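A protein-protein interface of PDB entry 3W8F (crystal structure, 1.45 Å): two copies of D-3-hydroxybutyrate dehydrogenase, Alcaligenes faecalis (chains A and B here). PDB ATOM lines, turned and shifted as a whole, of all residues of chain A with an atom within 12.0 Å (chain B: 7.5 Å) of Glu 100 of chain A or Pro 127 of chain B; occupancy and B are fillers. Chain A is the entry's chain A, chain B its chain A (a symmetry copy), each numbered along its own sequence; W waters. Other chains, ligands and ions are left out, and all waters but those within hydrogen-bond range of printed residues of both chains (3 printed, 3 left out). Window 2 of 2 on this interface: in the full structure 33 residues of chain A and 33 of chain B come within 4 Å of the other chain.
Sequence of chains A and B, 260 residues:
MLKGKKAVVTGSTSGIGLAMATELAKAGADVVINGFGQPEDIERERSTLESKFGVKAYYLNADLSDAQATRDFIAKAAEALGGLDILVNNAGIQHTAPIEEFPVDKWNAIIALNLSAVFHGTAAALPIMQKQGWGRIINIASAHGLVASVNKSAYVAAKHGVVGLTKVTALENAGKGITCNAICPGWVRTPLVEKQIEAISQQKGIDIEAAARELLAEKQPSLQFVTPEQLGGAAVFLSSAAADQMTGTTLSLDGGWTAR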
ATOM      1  N   HIS A  95     -16.546  17.368  -0.378  1.00  0.00           N
ATOM      2  CA  HIS A  95     -17.738  16.838   0.294  1.00  0.00           C
ATOM      3  C   HIS A  95     -17.938  17.574   1.557  1.00  0.00           C
ATOM      4  O   HIS A  95     -16.965  17.759   2.296  1.00  0.00           O
ATOM      5  CB  HIS A  95     -17.506  15.359   0.648  1.00  0.00           C
ATOM      6  CG  HIS A  95     -18.700  14.736   1.280  1.00  0.00           C
ATOM      7  ND1 HIS A  95     -19.753  14.280   0.519  1.00  0.00           N
ATOM      8  CD2 HIS A  95     -19.006  14.589   2.573  1.00  0.00           C
ATOM      9  CE1 HIS A  95     -20.678  13.828   1.366  1.00  0.00           C
ATOM     10  NE2 HIS A  95     -20.286  14.050   2.605  1.00  0.00           N
ATOM     11  N   THR A  96     -19.140  18.074   1.826  1.00  0.00           N
ATOM     12  CA  THR A  96     -19.363  18.866   3.031  1.00  0.00           C
ATOM     13  C   THR A  96     -20.255  18.164   4.035  1.00  0.00           C
ATOM     14  O   THR A  96     -21.311  17.591   3.711  1.00  0.00           O
ATOM     15  CB  THR A  96     -19.960  20.264   2.747  1.00  0.00           C
ATOM     16  OG1 THR A  96     -21.308  20.096   2.329  1.00  0.00           O
ATOM     17  CG2 THR A  96     -19.101  21.021   1.725  1.00  0.00           C
ATOM     18  N   ALA A  97     -19.809  18.130   5.261  1.00  0.00           N
ATOM     19  CA  ALA A  97     -20.551  17.531   6.418  1.00  0.00           C
ATOM     20  C   ALA A  97     -19.800  17.857   7.681  1.00  0.00           C
ATOM     21  O   ALA A  97     -18.573  18.027   7.634  1.00  0.00           O
ATOM     22  CB  ALA A  97     -20.561  16.000   6.300  1.00  0.00           C
ATOM     23  N   PRO A  98     -20.471  17.938   8.832  1.00  0.00           N
ATOM     24  CA  PRO A  98     -19.648  18.195  10.043  1.00  0.00           C
ATOM     25  C   PRO A  98     -18.838  16.969  10.416  1.00  0.00           C
ATOM     26  O   PRO A  98     -19.084  15.821   9.946  1.00  0.00           O
ATOM     27  CB  PRO A  98     -20.664  18.525  11.122  1.00  0.00           C
ATOM     28  CG  PRO A  98     -21.907  17.779  10.642  1.00  0.00           C
ATOM     29  CD  PRO A  98     -21.875  17.654   9.151  1.00  0.00           C
ATOM     30  N   ILE A  99     -17.786  17.211  11.138  1.00  0.00           N
ATOM     31  CA  ILE A  99     -16.775  16.151  11.391  1.00  0.00           C
ATOM     32  C   ILE A  99     -17.430  14.846  11.906  1.00  0.00           C
ATOM     33  O   ILE A  99     -17.071  13.769  11.422  1.00  0.00           O
ATOM     34  CB  ILE A  99     -15.706  16.671  12.409  1.00  0.00           C
ATOM     35  CG1 ILE A  99     -14.810  17.659  11.689  1.00  0.00           C
ATOM     36  CG2 ILE A  99     -14.918  15.461  12.939  1.00  0.00           C
ATOM     37  CD1 ILE A  99     -14.014  18.578  12.712  1.00  0.00           C
ATOM     38  N   GLU A 100     -18.287  14.919  12.907  1.00  0.00           N
ATOM     39  CA  GLU A 100     -18.834  13.691  13.497  1.00  0.00           C
ATOM     40  C   GLU A 100     -19.735  12.987  12.549  1.00  0.00           C
ATOM     41  O   GLU A 100     -20.027  11.795  12.874  1.00  0.00           O
ATOM     42  CB  GLU A 100     -19.534  14.053  14.817  1.00  0.00           C
ATOM     43  CG  GLU A 100     -20.734  14.947  14.744  1.00  0.00           C
ATOM     44  CD  GLU A 100     -20.472  16.423  14.686  1.00  0.00           C
ATOM     45  OE1 GLU A 100     -19.342  16.839  14.535  1.00  0.00           O
ATOM     46  OE2 GLU A 100     -21.438  17.194  14.783  1.00  0.00           O
ATOM     47  N   GLU A 101     -20.187  13.567  11.424  1.00  0.00           N
ATOM     48  CA  GLU A 101     -20.976  12.852  10.456  1.00  0.00           C
ATOM     49  C   GLU A 101     -20.211  12.700   9.151  1.00  0.00           C
ATOM     50  O   GLU A 101     -20.770  12.259   8.153  1.00  0.00           O
ATOM     51  CB  GLU A 101     -22.216  13.660  10.099  1.00  0.00           C
ATOM     52  CG  GLU A 101     -23.172  13.922  11.155  1.00  0.00           C
ATOM     53  CD  GLU A 101     -24.323  14.694  10.553  1.00  0.00           C
ATOM     54  OE1 GLU A 101     -25.085  14.134   9.716  1.00  0.00           O
ATOM     55  OE2 GLU A 101     -24.407  15.870  10.869  1.00  0.00           O
ATOM     56  N   PHE A 102     -18.928  13.008   9.100  1.00  0.00           N
ATOM     57  CA  PHE A 102     -18.239  13.032   7.846  1.00  0.00           C
ATOM     58  C   PHE A 102     -17.884  11.630   7.424  1.00  0.00           C
ATOM     59  O   PHE A 102     -17.243  10.919   8.190  1.00  0.00           O
ATOM     60  CB  PHE A 102     -16.942  13.897   8.024  1.00  0.00           C
ATOM     61  CG  PHE A 102     -16.426  14.420   6.718  1.00  0.00           C
ATOM     62  CD1 PHE A 102     -15.694  13.587   5.825  1.00  0.00           C
ATOM     63  CD2 PHE A 102     -16.673  15.732   6.346  1.00  0.00           C
ATOM     64  CE1 PHE A 102     -15.233  14.062   4.609  1.00  0.00           C
ATOM     65  CE2 PHE A 102     -16.252  16.181   5.095  1.00  0.00           C
ATOM     66  CZ  PHE A 102     -15.494  15.376   4.249  1.00  0.00           C
ATOM     67  N   PRO A 103     -18.316  11.177   6.243  1.00  0.00           N
ATOM     68  CA  PRO A 103     -18.134   9.742   5.970  1.00  0.00           C
ATOM     69  C   PRO A 103     -16.619   9.362   5.919  1.00  0.00           C
ATOM     70  O   PRO A 103     -15.823  10.110   5.289  1.00  0.00           O
ATOM     71  CB  PRO A 103     -18.777   9.583   4.575  1.00  0.00           C
ATOM     72  CG  PRO A 103     -19.811  10.691   4.502  1.00  0.00           C
ATOM     73  CD  PRO A 103     -19.140  11.881   5.242  1.00  0.00           C
ATOM     74  N   VAL A 104     -16.259   8.275   6.552  1.00  0.00           N
ATOM     75  CA  VAL A 104     -14.896   7.806   6.563  1.00  0.00           C
ATOM     76  C   VAL A 104     -14.415   7.614   5.121  1.00  0.00           C
ATOM     77  O   VAL A 104     -13.245   7.959   4.768  1.00  0.00           O
ATOM     78  CB  VAL A 104     -14.787   6.572   7.383  1.00  0.00           C
ATOM     79  CG1 VAL A 104     -13.436   5.863   7.143  1.00  0.00           C
ATOM     80  CG2 VAL A 104     -14.929   6.907   8.860  1.00  0.00           C
ATOM     81  N   ASP A 105     -15.251   7.054   4.237  1.00  0.00           N
ATOM     82  CA  ASP A 105     -14.827   6.854   2.865  1.00  0.00           C
ATOM     83  C   ASP A 105     -14.592   8.184   2.111  1.00  0.00           C
ATOM     84  O   ASP A 105     -13.763   8.239   1.215  1.00  0.00           O
ATOM     85  CB  ASP A 105     -15.865   5.990   2.108  1.00  0.00           C
ATOM     86  CG  ASP A 105     -17.257   6.480   2.309  1.00  0.00           C
ATOM     87  OD1 ASP A 105     -17.777   6.298   3.451  1.00  0.00           O
ATOM     88  OD2 ASP A 105     -17.779   7.091   1.341  1.00  0.00           O
ATOM     89  N   LYS A 106     -15.346   9.242   2.492  1.00  0.00           N
ATOM     90  CA  LYS A 106     -15.157  10.527   1.840  1.00  0.00           C
ATOM     91  C   LYS A 106     -13.834  11.176   2.389  1.00  0.00           C
ATOM     92  O   LYS A 106     -13.121  11.811   1.616  1.00  0.00           O
ATOM     93  CB  LYS A 106     -16.347  11.473   2.055  1.00  0.00           C
ATOM     94  CG  LYS A 106     -17.619  11.050   1.232  1.00  0.00           C
ATOM     95  CD  LYS A 106     -17.331  11.320  -0.201  1.00  0.00           C
ATOM     96  CE  LYS A 106     -18.575  10.803  -0.999  1.00  0.00           C
ATOM     97  NZ  LYS A 106     -18.306  11.275  -2.395  1.00  0.00           N
ATOM     98  N   TRP A 107     -13.588  11.050   3.679  1.00  0.00           N
ATOM     99  CA  TRP A 107     -12.249  11.475   4.166  1.00  0.00           C
ATOM    100  C   TRP A 107     -11.183  10.782   3.380  1.00  0.00           C
ATOM    101  O   TRP A 107     -10.298  11.455   2.872  1.00  0.00           O
ATOM    102  CB  TRP A 107     -12.151  11.161   5.675  1.00  0.00           C
ATOM    103  CG  TRP A 107     -10.780  11.339   6.186  1.00  0.00           C
ATOM    104  CD1 TRP A 107      -9.784  10.408   6.210  1.00  0.00           C
ATOM    105  CD2 TRP A 107     -10.210  12.535   6.744  1.00  0.00           C
ATOM    106  NE1 TRP A 107      -8.606  10.945   6.689  1.00  0.00           N
ATOM    107  CE2 TRP A 107      -8.854  12.253   7.020  1.00  0.00           C
ATOM    108  CE3 TRP A 107     -10.715  13.804   7.080  1.00  0.00           C
ATOM    109  CZ2 TRP A 107      -7.955  13.206   7.569  1.00  0.00           C
ATOM    110  CZ3 TRP A 107      -9.754  14.770   7.618  1.00  0.00           C
ATOM    111  CH2 TRP A 107      -8.415  14.411   7.820  1.00  0.00           C
ATOM    112  N   SER A 149     -13.143  26.588   6.930  1.00  0.00           N
ATOM    113  CA  SER A 149     -14.584  26.835   7.024  1.00  0.00           C
ATOM    114  C   SER A 149     -15.218  25.631   7.636  1.00  0.00           C
ATOM    115  O   SER A 149     -14.648  24.519   7.616  1.00  0.00           O
ATOM    116  CB  SER A 149     -15.264  27.006   5.676  1.00  0.00           C
ATOM    117  OG  SER A 149     -14.798  28.175   5.001  1.00  0.00           O
ATOM    118  N   VAL A 150     -16.421  25.780   8.159  1.00  0.00           N
ATOM    119  CA  VAL A 150     -17.115  24.637   8.758  1.00  0.00           C
ATOM    120  C   VAL A 150     -17.443  23.631   7.664  1.00  0.00           C
ATOM    121  O   VAL A 150     -17.580  23.908   6.477  1.00  0.00           O
ATOM    122  CB  VAL A 150     -18.443  25.078   9.438  1.00  0.00           C
ATOM    123  CG1 VAL A 150     -18.161  26.022  10.607  1.00  0.00           C
ATOM    124  CG2 VAL A 150     -19.397  25.790   8.451  1.00  0.00           C
ATOM    125  N   ASN A 151     -17.500  22.375   8.150  1.00  0.00           N
ATOM    126  CA  ASN A 151     -18.042  21.284   7.354  1.00  0.00           C
ATOM    127  C   ASN A 151     -17.162  20.813   6.219  1.00  0.00           C
ATOM    128  O   ASN A 151     -17.565  20.041   5.371  1.00  0.00           O
ATOM    129  CB  ASN A 151     -19.495  21.508   6.924  1.00  0.00           C
ATOM    130  CG  ASN A 151     -20.396  21.676   8.120  1.00  0.00           C
ATOM    131  OD1 ASN A 151     -20.126  21.342   9.222  1.00  0.00           O
ATOM    132  ND2 ASN A 151     -21.473  22.461   7.850  1.00  0.00           N
ATOM    133  N   LYS A 152     -15.880  21.217   6.284  1.00  0.00           N
ATOM    134  CA  LYS A 152     -14.914  20.877   5.247  1.00  0.00           C
ATOM    135  C   LYS A 152     -13.684  20.297   5.826  1.00  0.00           C
ATOM    136  O   LYS A 152     -12.570  20.541   5.347  1.00  0.00           O
ATOM    137  CB  LYS A 152     -14.611  22.104   4.398  1.00  0.00           C
ATOM    138  CG  LYS A 152     -15.839  22.450   3.526  1.00  0.00           C
ATOM    139  CD  LYS A 152     -15.558  23.716   2.638  1.00  0.00           C
ATOM    140  CE  LYS A 152     -16.760  23.899   1.739  1.00  0.00           C
ATOM    141  NZ  LYS A 152     -16.530  25.077   0.841  1.00  0.00           N
ATOM    142  N   SER A 153     -13.810  19.474   6.874  1.00  0.00           N
ATOM    143  CA  SER A 153     -12.622  18.915   7.529  1.00  0.00           C
ATOM    144  C   SER A 153     -11.624  18.275   6.586  1.00  0.00           C
ATOM    145  O   SER A 153     -10.420  18.556   6.594  1.00  0.00           O
ATOM    146  CB  SER A 153     -12.987  17.960   8.655  1.00  0.00           C
ATOM    147  OG  SER A 153     -13.850  16.891   8.138  1.00  0.00           O
ATOM    148  N   ALA A 154     -12.080  17.313   5.767  1.00  0.00           N
ATOM    149  CA  ALA A 154     -11.142  16.626   4.915  1.00  0.00           C
ATOM    150  C   ALA A 154     -10.488  17.551   3.909  1.00  0.00           C
ATOM    151  O   ALA A 154      -9.285  17.406   3.644  1.00  0.00           O
ATOM    152  CB  ALA A 154     -11.875  15.408   4.217  1.00  0.00           C
ATOM    153  N   ARG B  71     -11.666   4.887  16.281  1.00  0.00           N
ATOM    154  CA  ARG B  71     -12.986   5.214  16.788  1.00  0.00           C
ATOM    155  C   ARG B  71     -13.422   4.280  17.971  1.00  0.00           C
ATOM    156  O   ARG B  71     -14.006   4.753  18.937  1.00  0.00           O
ATOM    157  CB  ARG B  71     -14.006   5.092  15.637  1.00  0.00           C
ATOM    158  CG  ARG B  71     -13.695   6.245  14.643  1.00  0.00           C
ATOM    159  CD  ARG B  71     -14.404   6.026  13.262  1.00  0.00           C
ATOM    160  NE  ARG B  71     -14.147   7.202  12.393  1.00  0.00           N
ATOM    161  CZ  ARG B  71     -14.972   8.234  12.260  1.00  0.00           C
ATOM    162  NH1 ARG B  71     -16.192   8.277  12.753  1.00  0.00           N
ATOM    163  NH2 ARG B  71     -14.527   9.244  11.525  1.00  0.00           N
ATOM    164  N   ILE B  74     -11.675   5.441  21.222  1.00  0.00           N
ATOM    165  CA  ILE B  74     -12.291   6.503  21.915  1.00  0.00           C
ATOM    166  C   ILE B  74     -13.521   5.998  22.669  1.00  0.00           C
ATOM    167  O   ILE B  74     -13.743   6.420  23.781  1.00  0.00           O
ATOM    168  CB  ILE B  74     -12.698   7.599  20.897  1.00  0.00           C
ATOM    169  CG1 ILE B  74     -11.410   8.281  20.291  1.00  0.00           C
ATOM    170  CG2 ILE B  74     -13.582   8.660  21.589  1.00  0.00           C
ATOM    171  CD1 ILE B  74     -10.542   9.023  21.343  1.00  0.00           C
ATOM    172  N   PHE B 119      -8.398  13.064  12.849  1.00  0.00           N
ATOM    173  CA  PHE B 119      -9.755  13.157  12.395  1.00  0.00           C
ATOM    174  C   PHE B 119     -10.650  12.087  13.065  1.00  0.00           C
ATOM    175  O   PHE B 119     -11.731  12.425  13.592  1.00  0.00           O
ATOM    176  CB  PHE B 119      -9.793  13.003  10.858  1.00  0.00           C
ATOM    177  CG  PHE B 119     -11.139  12.749  10.347  1.00  0.00           C
ATOM    178  CD1 PHE B 119     -12.092  13.792  10.284  1.00  0.00           C
ATOM    179  CD2 PHE B 119     -11.432  11.520   9.835  1.00  0.00           C
ATOM    180  CE1 PHE B 119     -13.385  13.517   9.751  1.00  0.00           C
ATOM    181  CE2 PHE B 119     -12.741  11.220   9.290  1.00  0.00           C
ATOM    182  CZ  PHE B 119     -13.700  12.232   9.258  1.00  0.00           C
ATOM    183  N   GLY B 121     -10.208  10.293  15.775  1.00  0.00           N
ATOM    184  CA  GLY B 121     -10.342  10.451  17.218  1.00  0.00           C
ATOM    185  C   GLY B 121     -11.245  11.618  17.561  1.00  0.00           C
ATOM    186  O   GLY B 121     -12.112  11.516  18.450  1.00  0.00           O
ATOM    187  N   THR B 122     -11.105  12.744  16.832  1.00  0.00           N
ATOM    188  CA  THR B 122     -11.989  13.920  17.042  1.00  0.00           C
ATOM    189  C   THR B 122     -13.421  13.549  16.731  1.00  0.00           C
ATOM    190  O   THR B 122     -14.324  13.931  17.475  1.00  0.00           O
ATOM    191  CB  THR B 122     -11.475  15.035  16.119  1.00  0.00           C
ATOM    192  OG1 THR B 122     -10.148  15.427  16.562  1.00  0.00           O
ATOM    193  CG2 THR B 122     -12.401  16.264  16.204  1.00  0.00           C
ATOM    194  N   ALA B 123     -13.639  12.863  15.591  1.00  0.00           N
ATOM    195  CA  ALA B 123     -15.020  12.541  15.247  1.00  0.00           C
ATOM    196  C   ALA B 123     -15.667  11.700  16.288  1.00  0.00           C
ATOM    197  O   ALA B 123     -16.888  11.837  16.569  1.00  0.00           O
ATOM    198  CB  ALA B 123     -15.020  11.788  13.896  1.00  0.00           C
ATOM    199  N   ALA B 124     -14.932  10.768  16.892  1.00  0.00           N
ATOM    200  CA  ALA B 124     -15.554   9.916  17.899  1.00  0.00           C
ATOM    201  C   ALA B 124     -15.723  10.622  19.201  1.00  0.00           C
ATOM    202  O   ALA B 124     -16.670  10.347  19.966  1.00  0.00           O
ATOM    203  CB  ALA B 124     -14.637   8.644  18.149  1.00  0.00           C
ATOM    204  N   ALA B 125     -14.851  11.554  19.566  1.00  0.00           N
ATOM    205  CA  ALA B 125     -14.991  12.271  20.834  1.00  0.00           C
ATOM    206  C   ALA B 125     -16.026  13.360  20.804  1.00  0.00           C
ATOM    207  O   ALA B 125     -16.631  13.698  21.845  1.00  0.00           O
ATOM    208  CB  ALA B 125     -13.654  12.870  21.217  1.00  0.00           C
ATOM    209  N   LEU B 126     -16.213  14.019  19.647  1.00  0.00           N
ATOM    210  CA  LEU B 126     -17.089  15.213  19.656  1.00  0.00           C
ATOM    211  C   LEU B 126     -18.480  15.006  20.150  1.00  0.00           C
ATOM    212  O   LEU B 126     -18.941  15.898  20.877  1.00  0.00           O
ATOM    213  CB  LEU B 126     -17.068  15.877  18.286  1.00  0.00           C
ATOM    214  CG  LEU B 126     -15.889  16.755  17.904  1.00  0.00           C
ATOM    215  CD1 LEU B 126     -15.924  17.155  16.416  1.00  0.00           C
ATOM    216  CD2 LEU B 126     -15.905  18.030  18.833  1.00  0.00           C
ATOM    217  N   PRO B 127     -19.171  13.896  19.820  1.00  0.00           N
ATOM    218  CA  PRO B 127     -20.540  13.804  20.303  1.00  0.00           C
ATOM    219  C   PRO B 127     -20.635  13.785  21.818  1.00  0.00           C
ATOM    220  O   PRO B 127     -21.589  14.320  22.388  1.00  0.00           O
ATOM    221  CB  PRO B 127     -21.035  12.511  19.674  1.00  0.00           C
ATOM    222  CG  PRO B 127     -20.194  12.424  18.357  1.00  0.00           C
ATOM    223  CD  PRO B 127     -18.853  12.883  18.785  1.00  0.00           C
ATOM    224  N   ILE B 128     -19.635  13.230  22.477  1.00  0.00           N
ATOM    225  CA  ILE B 128     -19.596  13.155  23.937  1.00  0.00           C
ATOM    226  C   ILE B 128     -19.451  14.535  24.473  1.00  0.00           C
ATOM    227  O   ILE B 128     -20.225  15.017  25.361  1.00  0.00           O
ATOM    228  CB  ILE B 128     -18.452  12.226  24.328  1.00  0.00           C
ATOM    229  CG1 ILE B 128     -18.685  10.828  23.742  1.00  0.00           C
ATOM    230  CG2 ILE B 128     -18.281  12.208  25.873  1.00  0.00           C
ATOM    231  CD1 ILE B 128     -17.397   9.896  23.906  1.00  0.00           C
ATOM    232  N   MET B 129     -18.503  15.300  23.913  1.00  0.00           N
ATOM    233  CA  MET B 129     -18.306  16.679  24.361  1.00  0.00           C
ATOM    234  C   MET B 129     -19.481  17.589  24.016  1.00  0.00           C
ATOM    235  O   MET B 129     -19.797  18.467  24.835  1.00  0.00           O
ATOM    236  CB  MET B 129     -16.991  17.206  23.713  1.00  0.00           C
ATOM    237  CG  MET B 129     -15.772  16.405  24.147  1.00  0.00           C
ATOM    238  SD  MET B 129     -14.347  17.079  23.236  1.00  0.00           S
ATOM    239  CE  MET B 129     -13.063  16.041  24.021  1.00  0.00           C
ATOM    240  N   GLN B 130     -20.117  17.364  22.881  1.00  0.00           N
ATOM    241  CA  GLN B 130     -21.274  18.213  22.496  1.00  0.00           C
ATOM    242  C   GLN B 130     -22.437  17.974  23.444  1.00  0.00           C
ATOM    243  O   GLN B 130     -23.100  18.941  23.834  1.00  0.00           O
ATOM    244  CB  GLN B 130     -21.633  17.881  21.091  1.00  0.00           C
ATOM    245  CG  GLN B 130     -20.585  18.419  20.046  1.00  0.00           C
ATOM    246  CD  GLN B 130     -20.749  17.831  18.699  1.00  0.00           C
ATOM    247  OE1 GLN B 130     -21.377  16.743  18.502  1.00  0.00           O
ATOM    248  NE2 GLN B 130     -20.128  18.438  17.707  1.00  0.00           N
ATOM    249  N   LYS B 131     -22.620  16.751  23.844  1.00  0.00           N
ATOM    250  CA  LYS B 131     -23.770  16.444  24.778  1.00  0.00           C
ATOM    251  C   LYS B 131     -23.515  17.093  26.090  1.00  0.00           C
ATOM    252  O   LYS B 131     -24.476  17.556  26.716  1.00  0.00           O
ATOM    253  CB  LYS B 131     -23.890  14.945  24.916  1.00  0.00           C
ATOM    254  CG  LYS B 131     -25.060  14.472  25.710  1.00  0.00           C
ATOM    255  CD  LYS B 131     -25.306  12.953  25.472  1.00  0.00           C
ATOM    256  CE  LYS B 131     -25.015  12.048  26.724  1.00  0.00           C
ATOM    257  NZ  LYS B 131     -26.087  11.932  27.795  1.00  0.00           N
ATOM    258  N   GLN B 132     -22.332  17.197  26.588  1.00  0.00           N
ATOM    259  CA  GLN B 132     -22.081  17.844  27.886  1.00  0.00           C
ATOM    260  C   GLN B 132     -21.844  19.304  27.869  1.00  0.00           C
ATOM    261  O   GLN B 132     -21.800  19.936  28.916  1.00  0.00           O
ATOM    262  CB  GLN B 132     -21.003  17.170  28.596  1.00  0.00           C
ATOM    263  CG  GLN B 132     -19.659  17.410  27.964  1.00  0.00           C
ATOM    264  CD  GLN B 132     -18.653  16.300  28.273  1.00  0.00           C
ATOM    265  OE1 GLN B 132     -17.413  16.369  27.906  1.00  0.00           O
ATOM    266  NE2 GLN B 132     -19.179  15.205  28.830  1.00  0.00           N
ATOM    267  N   GLY B 133     -21.613  19.828  26.659  1.00  0.00           N
ATOM    268  CA  GLY B 133     -21.359  21.277  26.579  1.00  0.00           C
ATOM    269  C   GLY B 133     -20.013  21.777  27.025  1.00  0.00           C
ATOM    270  O   GLY B 133     -19.854  22.903  27.415  1.00  0.00           O
ATOM    271  N   GLU B 172     -16.561  24.491  13.768  1.00  0.00           N
ATOM    272  CA  GLU B 172     -17.809  23.734  13.838  1.00  0.00           C
ATOM    273  C   GLU B 172     -18.324  23.698  15.244  1.00  0.00           C
ATOM    274  O   GLU B 172     -19.547  23.479  15.400  1.00  0.00           O
ATOM    275  CB  GLU B 172     -17.540  22.301  13.374  1.00  0.00           C
ATOM    276  CG  GLU B 172     -17.337  22.204  11.857  1.00  0.00           C
ATOM    277  CD  GLU B 172     -17.149  20.763  11.370  1.00  0.00           C
ATOM    278  OE1 GLU B 172     -17.356  19.769  12.163  1.00  0.00           O
ATOM    279  OE2 GLU B 172     -16.824  20.613  10.175  1.00  0.00           O
ATOM    280  N   ASN B 173     -17.508  23.946  16.236  1.00  0.00           N
ATOM    281  CA  ASN B 173     -17.929  23.805  17.642  1.00  0.00           C
ATOM    282  C   ASN B 173     -17.883  25.096  18.399  1.00  0.00           C
ATOM    283  O   ASN B 173     -17.958  25.166  19.612  1.00  0.00           O
ATOM    284  CB  ASN B 173     -17.134  22.680  18.291  1.00  0.00           C
ATOM    285  CG  ASN B 173     -17.487  21.377  17.632  1.00  0.00           C
ATOM    286  OD1 ASN B 173     -16.804  20.875  16.720  1.00  0.00           O
ATOM    287  ND2 ASN B 173     -18.613  20.833  18.025  1.00  0.00           N
ATOM    288  N   LYS B 176     -19.838  26.318  21.687  1.00  0.00           N
ATOM    289  CA  LYS B 176     -20.517  25.154  22.289  1.00  0.00           C
ATOM    290  C   LYS B 176     -19.780  24.781  23.589  1.00  0.00           C
ATOM    291  O   LYS B 176     -20.209  23.764  24.218  1.00  0.00           O
ATOM    292  CB  LYS B 176     -20.482  23.913  21.378  1.00  0.00           C
ATOM    293  CG  LYS B 176     -21.262  24.104  20.124  1.00  0.00           C
ATOM    294  CD  LYS B 176     -21.173  22.763  19.311  1.00  0.00           C
ATOM    295  CE  LYS B 176     -21.896  22.953  17.974  1.00  0.00           C
ATOM    296  NZ  LYS B 176     -21.725  21.625  17.218  1.00  0.00           N
ATOM    297  N   ILE B 178     -16.675  23.889  23.639  1.00  0.00           N
ATOM    298  CA  ILE B 178     -15.591  22.985  23.117  1.00  0.00           C
ATOM    299  C   ILE B 178     -14.563  23.772  22.397  1.00  0.00           C
ATOM    300  O   ILE B 178     -14.979  24.563  21.492  1.00  0.00           O
ATOM    301  CB  ILE B 178     -16.154  21.981  22.166  1.00  0.00           C
ATOM    302  CG1 ILE B 178     -17.241  21.139  22.905  1.00  0.00           C
ATOM    303  CG2 ILE B 178     -15.035  21.032  21.637  1.00  0.00           C
ATOM    304  CD1 ILE B 178     -18.085  20.308  21.977  1.00  0.00           C
HETATM  305  O   HOH W   1     -16.049  18.628   8.526  1.00  0.00           O
HETATM  306  O   HOH W   2     -16.740  10.968  10.863  1.00  0.00           O
HETATM  307  O   HOH W   3     -20.808  20.171  14.720  1.00  0.00           O
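The side-chain carboxylate (OE1) of Glu 172 of chain B sits at hydrogen-bond distance from the backbone NH (N) of Ile 99 of chain A (2.8 Å).
OE2 of Glu 100 of chain A sits at hydrogen-bond distance from NE2 of Gln 130 of chain B (3.4 Å).
The backbone NH of Asn 151 of chain A is in hydrogen-bond range of the side-chain carboxylate of Glu 172 of chain B, at 2.8 Å.
The side-chain amide nitrogen of Gln 130 of chain B sits close to the side-chain amide nitrogen of Asn 173 of chain B, at 2.9 Å.
The backbone carbonyl oxygen of Glu 172 of chain B sits at hydrogen-bond distance from the side-chain amino group of Lys 176 of chain B.
Among the printed residues, pairs that only touch across the chains: Pro 98 of chain A with Glu 172 of chain B (3.5 Å), Ile 99 of chain A with Ala 123 of chain B (3.7 Å), Ile 99 of chain A with Leu 126 of chain B (3.996 Å), Glu 100 of chain A with Ala 123 of chain B (3.9 Å), Glu 100 of chain A with Leu 126 of chain B (3.9 Å), Glu 100 of chain A with Pro 127 of chain B (3.95 Å), Phe 102 of chain A with Phe 119 of chain B (3.8 Å), Val 104 of chain A with Arg 71 of chain B (3.6 Å), Trp 107 of chain A with Phe 119 of chain B (3.5 Å), Val 150 of chain A with Glu 172 of chain B (3.9 Å) and Ser 153 of chain A with Phe 119 of chain B (3.8 Å).
Printed residues of chain B within 4 Å of Pro 98 of chain A: Glu 172.
Of the printed residues of chain B, Val 104 of chain A touches Arg 71.
Of the printed residues of chain B, Asn 151 of chain A touches Glu 172.
No residue of chain A comes within 4 Å of Ala 124 of chain B.
Pro 127 of chain B touches just one residue of chain A: Glu 100 (3.95 Å).
Of chain A, only Glu 100 comes within 4 Å of Gln 130 of chain B.
Lys 131 of chain B touches none of the printed residues of chain A.
Of the 20 printed residues of chain B, 7 touch a printed residue of chain A.
Hydrophobic or aromatic side chains of chain B that line the printed part of chain A: Phe 119, Ala 123, Leu 126 and Pro 127.
Of the 19 printed residues of chain A, 9 touch a printed residue of chain B.
Hydrophobic or aromatic side chains of chain A within 4 Å of the printed part of chain B: Pro 98, Ile 99, Phe 102, Val 104, Trp 107 and Val 150.
Among the printed residues, 14 pairs touch across the chains.
No position is printed for both chains.
Water W2 lies within hydrogen-bond range of O of Phe 102 of chain A (2.7 Å), O of Ile 99 of chain A (2.9 Å) and NH2 of Arg 71 of chain B (2.9 Å).
Water W3 bridges the side-chain amino group (NZ) of Lys 176 of chain B (3.0 Å) and the side-chain carboxylate (OE2) of Glu 100 of chain A (3.0 Å).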
